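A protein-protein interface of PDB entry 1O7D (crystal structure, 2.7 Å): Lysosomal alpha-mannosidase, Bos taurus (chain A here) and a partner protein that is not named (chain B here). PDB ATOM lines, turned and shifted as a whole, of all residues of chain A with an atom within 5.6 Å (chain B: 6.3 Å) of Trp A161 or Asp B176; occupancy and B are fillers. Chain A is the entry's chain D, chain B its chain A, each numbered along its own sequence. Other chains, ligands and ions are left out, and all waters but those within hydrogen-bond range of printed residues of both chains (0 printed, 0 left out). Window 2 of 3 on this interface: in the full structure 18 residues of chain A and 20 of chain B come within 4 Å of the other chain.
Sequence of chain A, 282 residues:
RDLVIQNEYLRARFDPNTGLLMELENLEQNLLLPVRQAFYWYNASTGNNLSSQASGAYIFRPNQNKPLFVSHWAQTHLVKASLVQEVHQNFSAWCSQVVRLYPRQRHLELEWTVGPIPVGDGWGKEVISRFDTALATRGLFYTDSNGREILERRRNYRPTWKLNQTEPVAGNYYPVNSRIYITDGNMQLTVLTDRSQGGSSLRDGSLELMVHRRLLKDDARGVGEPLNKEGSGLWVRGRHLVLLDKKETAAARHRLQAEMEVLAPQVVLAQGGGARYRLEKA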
ATOM      1  N   ARG A 158       1.431  11.341  -7.074  1.00  0.00           N
ATOM      2  CA  ARG A 158       0.182  11.099  -7.767  1.00  0.00           C
ATOM      3  C   ARG A 158      -0.978  11.703  -7.011  1.00  0.00           C
ATOM      4  O   ARG A 158      -1.202  11.381  -5.859  1.00  0.00           O
ATOM      5  CB  ARG A 158      -0.062   9.604  -7.955  1.00  0.00           C
ATOM      6  CG  ARG A 158       0.893   8.937  -8.922  1.00  0.00           C
ATOM      7  CD  ARG A 158       0.758   9.468 -10.338  1.00  0.00           C
ATOM      8  NE  ARG A 158       1.750   8.860 -11.226  1.00  0.00           N
ATOM      9  CZ  ARG A 158       3.027   9.234 -11.309  1.00  0.00           C
ATOM     10  NH1 ARG A 158       3.498  10.232 -10.567  1.00  0.00           N
ATOM     11  NH2 ARG A 158       3.852   8.594 -12.126  1.00  0.00           N
ATOM     12  N   PRO A 159      -1.707  12.631  -7.646  1.00  0.00           N
ATOM     13  CA  PRO A 159      -2.868  13.291  -7.038  1.00  0.00           C
ATOM     14  C   PRO A 159      -3.910  12.268  -6.596  1.00  0.00           C
ATOM     15  O   PRO A 159      -4.508  12.374  -5.540  1.00  0.00           O
ATOM     16  CB  PRO A 159      -3.403  14.139  -8.182  1.00  0.00           C
ATOM     17  CG  PRO A 159      -2.139  14.565  -8.874  1.00  0.00           C
ATOM     18  CD  PRO A 159      -1.303  13.313  -8.893  1.00  0.00           C
ATOM     19  N   THR A 160      -4.096  11.266  -7.434  1.00  0.00           N
ATOM     20  CA  THR A 160      -5.082  10.222  -7.227  1.00  0.00           C
ATOM     21  C   THR A 160      -4.790   9.062  -6.269  1.00  0.00           C
ATOM     22  O   THR A 160      -5.731   8.484  -5.714  1.00  0.00           O
ATOM     23  CB  THR A 160      -5.477   9.690  -8.596  1.00  0.00           C
ATOM     24  OG1 THR A 160      -6.246  10.702  -9.264  1.00  0.00           O
ATOM     25  CG2 THR A 160      -6.258   8.399  -8.490  1.00  0.00           C
ATOM     26  N   TRP A 161      -3.527   8.683  -6.076  1.00  0.00           N
ATOM     27  CA  TRP A 161      -3.254   7.599  -5.125  1.00  0.00           C
ATOM     28  C   TRP A 161      -1.858   7.704  -4.510  1.00  0.00           C
ATOM     29  O   TRP A 161      -1.159   8.688  -4.708  1.00  0.00           O
ATOM     30  CB  TRP A 161      -3.458   6.231  -5.787  1.00  0.00           C
ATOM     31  CG  TRP A 161      -2.350   5.809  -6.684  1.00  0.00           C
ATOM     32  CD1 TRP A 161      -1.210   5.130  -6.332  1.00  0.00           C
ATOM     33  CD2 TRP A 161      -2.251   6.065  -8.088  1.00  0.00           C
ATOM     34  NE1 TRP A 161      -0.405   4.949  -7.438  1.00  0.00           N
ATOM     35  CE2 TRP A 161      -1.016   5.513  -8.529  1.00  0.00           C
ATOM     36  CE3 TRP A 161      -3.080   6.711  -9.018  1.00  0.00           C
ATOM     37  CZ2 TRP A 161      -0.594   5.586  -9.867  1.00  0.00           C
ATOM     38  CZ3 TRP A 161      -2.665   6.786 -10.342  1.00  0.00           C
ATOM     39  CH2 TRP A 161      -1.424   6.225 -10.756  1.00  0.00           C
ATOM     40  N   LYS A 162      -1.445   6.714  -3.735  1.00  0.00           N
ATOM     41  CA  LYS A 162      -0.124   6.797  -3.135  1.00  0.00           C
ATOM     42  C   LYS A 162       0.817   5.966  -3.964  1.00  0.00           C
ATOM     43  O   LYS A 162       0.930   4.761  -3.758  1.00  0.00           O
ATOM     44  CB  LYS A 162      -0.163   6.279  -1.717  1.00  0.00           C
ATOM     45  CG  LYS A 162       1.145   6.420  -0.966  1.00  0.00           C
ATOM     46  CD  LYS A 162       0.989   5.954   0.483  1.00  0.00           C
ATOM     47  CE  LYS A 162       2.296   6.077   1.274  1.00  0.00           C
ATOM     48  NZ  LYS A 162       2.706   7.519   1.406  1.00  0.00           N
ATOM     49  N   LEU A 163       1.490   6.619  -4.901  1.00  0.00           N
ATOM     50  CA  LEU A 163       2.427   5.977  -5.827  1.00  0.00           C
ATOM     51  C   LEU A 163       3.731   5.326  -5.326  1.00  0.00           C
ATOM     52  O   LEU A 163       4.493   5.925  -4.569  1.00  0.00           O
ATOM     53  CB  LEU A 163       2.823   6.991  -6.907  1.00  0.00           C
ATOM     54  CG  LEU A 163       4.003   6.555  -7.787  1.00  0.00           C
ATOM     55  CD1 LEU A 163       3.560   5.370  -8.654  1.00  0.00           C
ATOM     56  CD2 LEU A 163       4.485   7.714  -8.656  1.00  0.00           C
ATOM     57  N   ASN A 164       3.973   4.093  -5.760  1.00  0.00           N
ATOM     58  CA  ASN A 164       5.236   3.434  -5.446  1.00  0.00           C
ATOM     59  C   ASN A 164       5.997   3.534  -6.768  1.00  0.00           C
ATOM     60  O   ASN A 164       5.691   2.833  -7.741  1.00  0.00           O
ATOM     61  CB  ASN A 164       5.075   1.958  -5.076  1.00  0.00           C
ATOM     62  CG  ASN A 164       6.427   1.231  -4.984  1.00  0.00           C
ATOM     63  OD1 ASN A 164       7.310   1.643  -4.232  1.00  0.00           O
ATOM     64  ND2 ASN A 164       6.580   0.164  -5.769  1.00  0.00           N
ATOM     65  N   LEU B 172      -5.240   2.277 -17.939  1.00  0.00           N
ATOM     66  CA  LEU B 172      -4.934   3.193 -16.847  1.00  0.00           C
ATOM     67  C   LEU B 172      -3.825   2.541 -16.060  1.00  0.00           C
ATOM     68  O   LEU B 172      -3.640   1.331 -16.130  1.00  0.00           O
ATOM     69  CB  LEU B 172      -6.134   3.458 -15.931  1.00  0.00           C
ATOM     70  CG  LEU B 172      -6.629   2.443 -14.903  1.00  0.00           C
ATOM     71  CD1 LEU B 172      -7.635   3.107 -13.986  1.00  0.00           C
ATOM     72  CD2 LEU B 172      -7.241   1.257 -15.621  1.00  0.00           C
ATOM     73  N   ASP B 173      -3.079   3.348 -15.317  1.00  0.00           N
ATOM     74  CA  ASP B 173      -1.966   2.840 -14.534  1.00  0.00           C
ATOM     75  C   ASP B 173      -2.386   1.613 -13.736  1.00  0.00           C
ATOM     76  O   ASP B 173      -3.489   1.574 -13.179  1.00  0.00           O
ATOM     77  CB  ASP B 173      -1.456   3.911 -13.585  1.00  0.00           C
ATOM     78  CG  ASP B 173      -0.069   3.608 -13.089  1.00  0.00           C
ATOM     79  OD1 ASP B 173       0.125   2.483 -12.577  1.00  0.00           O
ATOM     80  OD2 ASP B 173       0.830   4.478 -13.218  1.00  0.00           O
ATOM     81  N   TYR B 174      -1.515   0.611 -13.662  1.00  0.00           N
ATOM     82  CA  TYR B 174      -1.886  -0.590 -12.928  1.00  0.00           C
ATOM     83  C   TYR B 174      -2.138  -0.322 -11.444  1.00  0.00           C
ATOM     84  O   TYR B 174      -3.067  -0.890 -10.876  1.00  0.00           O
ATOM     85  CB  TYR B 174      -0.848  -1.711 -13.113  1.00  0.00           C
ATOM     86  CG  TYR B 174       0.477  -1.457 -12.458  1.00  0.00           C
ATOM     87  CD1 TYR B 174       1.360  -0.503 -12.967  1.00  0.00           C
ATOM     88  CD2 TYR B 174       0.837  -2.135 -11.303  1.00  0.00           C
ATOM     89  CE1 TYR B 174       2.572  -0.224 -12.329  1.00  0.00           C
ATOM     90  CE2 TYR B 174       2.039  -1.869 -10.657  1.00  0.00           C
ATOM     91  CZ  TYR B 174       2.905  -0.910 -11.172  1.00  0.00           C
ATOM     92  OH  TYR B 174       4.087  -0.628 -10.510  1.00  0.00           O
ATOM     93  N   GLN B 175      -1.344   0.548 -10.820  1.00  0.00           N
ATOM     94  CA  GLN B 175      -1.547   0.838  -9.402  1.00  0.00           C
ATOM     95  C   GLN B 175      -2.857   1.580  -9.207  1.00  0.00           C
ATOM     96  O   GLN B 175      -3.544   1.360  -8.210  1.00  0.00           O
ATOM     97  CB  GLN B 175      -0.415   1.688  -8.814  1.00  0.00           C
ATOM     98  CG  GLN B 175       0.977   1.129  -8.991  1.00  0.00           C
ATOM     99  CD  GLN B 175       1.993   1.830  -8.106  1.00  0.00           C
ATOM    100  OE1 GLN B 175       1.806   2.980  -7.705  1.00  0.00           O
ATOM    101  NE2 GLN B 175       3.084   1.141  -7.807  1.00  0.00           N
ATOM    102  N   ASP B 176      -3.194   2.459 -10.151  1.00  0.00           N
ATOM    103  CA  ASP B 176      -4.434   3.221 -10.058  1.00  0.00           C
ATOM    104  C   ASP B 176      -5.611   2.262 -10.108  1.00  0.00           C
ATOM    105  O   ASP B 176      -6.533   2.370  -9.316  1.00  0.00           O
ATOM    106  CB  ASP B 176      -4.537   4.242 -11.206  1.00  0.00           C
ATOM    107  CG  ASP B 176      -5.647   5.291 -10.980  1.00  0.00           C
ATOM    108  OD1 ASP B 176      -5.991   5.546  -9.800  1.00  0.00           O
ATOM    109  OD2 ASP B 176      -6.160   5.871 -11.970  1.00  0.00           O
ATOM    110  N   LYS B 177      -5.563   1.315 -11.035  1.00  0.00           N
ATOM    111  CA  LYS B 177      -6.636   0.345 -11.176  1.00  0.00           C
ATOM    112  C   LYS B 177      -6.829  -0.456  -9.903  1.00  0.00           C
ATOM    113  O   LYS B 177      -7.946  -0.552  -9.394  1.00  0.00           O
ATOM    114  CB  LYS B 177      -6.341  -0.612 -12.329  1.00  0.00           C
ATOM    115  CG  LYS B 177      -7.528  -1.485 -12.712  1.00  0.00           C
ATOM    116  CD  LYS B 177      -7.251  -2.275 -13.972  1.00  0.00           C
ATOM    117  CE  LYS B 177      -8.487  -2.989 -14.486  1.00  0.00           C
ATOM    118  NZ  LYS B 177      -8.223  -3.737 -15.757  1.00  0.00           N
ATOM    119  N   LYS B 178      -5.743  -1.031  -9.395  1.00  0.00           N
ATOM    120  CA  LYS B 178      -5.787  -1.833  -8.180  1.00  0.00           C
ATOM    121  C   LYS B 178      -6.557  -1.097  -7.098  1.00  0.00           C
ATOM    122  O   LYS B 178      -7.512  -1.628  -6.532  1.00  0.00           O
ATOM    123  CB  LYS B 178      -4.373  -2.122  -7.677  1.00  0.00           C
ATOM    124  CG  LYS B 178      -4.340  -2.829  -6.319  1.00  0.00           C
ATOM    125  CD  LYS B 178      -3.009  -2.621  -5.542  1.00  0.00           C
ATOM    126  CE  LYS B 178      -2.975  -1.316  -4.695  1.00  0.00           C
ATOM    127  NZ  LYS B 178      -2.434  -0.085  -5.370  1.00  0.00           N
ATOM    128  N   VAL B 179      -6.141   0.132  -6.813  1.00  0.00           N
ATOM    129  CA  VAL B 179      -6.794   0.931  -5.789  1.00  0.00           C
ATOM    130  C   VAL B 179      -8.278   1.149  -6.098  1.00  0.00           C
ATOM    131  O   VAL B 179      -9.134   0.980  -5.227  1.00  0.00           O
ATOM    132  CB  VAL B 179      -6.124   2.311  -5.638  1.00  0.00           C
ATOM    133  CG1 VAL B 179      -6.655   3.011  -4.406  1.00  0.00           C
ATOM    134  CG2 VAL B 179      -4.630   2.157  -5.546  1.00  0.00           C
ATOM    135  N   ARG B 180      -8.583   1.508  -7.337  1.00  0.00           N
ATOM    136  CA  ARG B 180      -9.963   1.756  -7.714  1.00  0.00           C
ATOM    137  C   ARG B 180     -10.893   0.579  -7.475  1.00  0.00           C
ATOM    138  O   ARG B 180     -12.006   0.774  -6.982  1.00  0.00           O
ATOM    139  CB  ARG B 180     -10.044   2.227  -9.172  1.00  0.00           C
ATOM    140  CG  ARG B 180      -9.664   3.697  -9.334  1.00  0.00           C
ATOM    141  CD  ARG B 180      -9.633   4.161 -10.776  1.00  0.00           C
ATOM    142  NE  ARG B 180      -9.056   5.499 -10.891  1.00  0.00           N
ATOM    143  CZ  ARG B 180      -9.690   6.631 -10.591  1.00  0.00           C
ATOM    144  NH1 ARG B 180     -10.940   6.596 -10.162  1.00  0.00           N
ATOM    145  NH2 ARG B 180      -9.063   7.799 -10.697  1.00  0.00           N
ATOM    146  N   LYS B 181     -10.461  -0.634  -7.815  1.00  0.00           N
ATOM    147  CA  LYS B 181     -11.305  -1.811  -7.587  1.00  0.00           C
ATOM    148  C   LYS B 181     -11.490  -2.059  -6.087  1.00  0.00           C
ATOM    149  O   LYS B 181     -12.555  -2.498  -5.645  1.00  0.00           O
ATOM    150  CB  LYS B 181     -10.704  -3.067  -8.216  1.00  0.00           C
ATOM    151  CG  LYS B 181     -10.626  -3.057  -9.733  1.00  0.00           C
ATOM    152  CD  LYS B 181     -10.583  -4.481 -10.291  1.00  0.00           C
ATOM    153  CE  LYS B 181      -9.439  -5.316  -9.691  1.00  0.00           C
ATOM    154  NZ  LYS B 181      -9.309  -6.637 -10.386  1.00  0.00           N
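The side-chain amide oxygen (OE1) of Gln B175 is in hydrogen-bond range of the indole nitrogen (NE1) of Trp A161 (3.0 Å). The side-chain amide nitrogen of Gln B175 sits at hydrogen-bond distance from the backbone carbonyl oxygen of Asn A164 (3.1 Å).
The side-chain carboxylate (OD1) of Asp B173 lies within hydrogen-bond range of the backbone NH (N) of Gln B175 (3.0 Å). OH of Tyr B174 is in hydrogen-bond range of NE2 of Gln B175, at 3.4 Å. The side-chain amino group of Lys B178 is in hydrogen-bond range of the backbone carbonyl oxygen of Gln B175. The guanidinium group of Arg B180 is in salt-bridge range of the side-chain carboxylate of Asp B176, 3.1 Å away.
Asp B176 touches Thr A160 (OD1 to CG2, 3.2 Å). Thr A160 touches Arg B180 (CG2 to NH2, 3.6 Å). Trp A161 touches Asp B173. Trp A161 touches Asp B176 (CE3 to OD1, 3.2 Å). OE1 of Gln B175 touches CD1 of Leu A163 (3.1 Å).
Of chain B, only Asp B173, Gln B175 and Asp B176 come within 4 Å of Trp A161. Of chain A, only Thr A160 and Trp A161 come within 4 Å of Asp B176. Printed residues of chain B within 4 Å of Thr A160: Asp B176 (3.2 Å) and Arg B180 (3.6 Å). Printed residues of chain B within 4 Å of Leu A163: Gln B175. Printed residues of chain B within 4 Å of Asn A164: Gln B175 (3.1 Å). Of the printed residues of chain A, Arg B180 touches Thr A160. Printed residues of chain A within 4 Å of Asp B173: Trp A161 (3.7 Å). The nearest residue of chain B that does not touch Trp A161 is Val B179 (4.2 Å).
Printed residues of chain B that touch a printed residue of chain A: Asp B173, Gln B175, Asp B176 and Arg B180. Hydrophobic or aromatic side chains of chain A that line the printed part of chain B: Trp A161 and Leu A163. Among the printed residues, 7 pairs touch across the chains.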
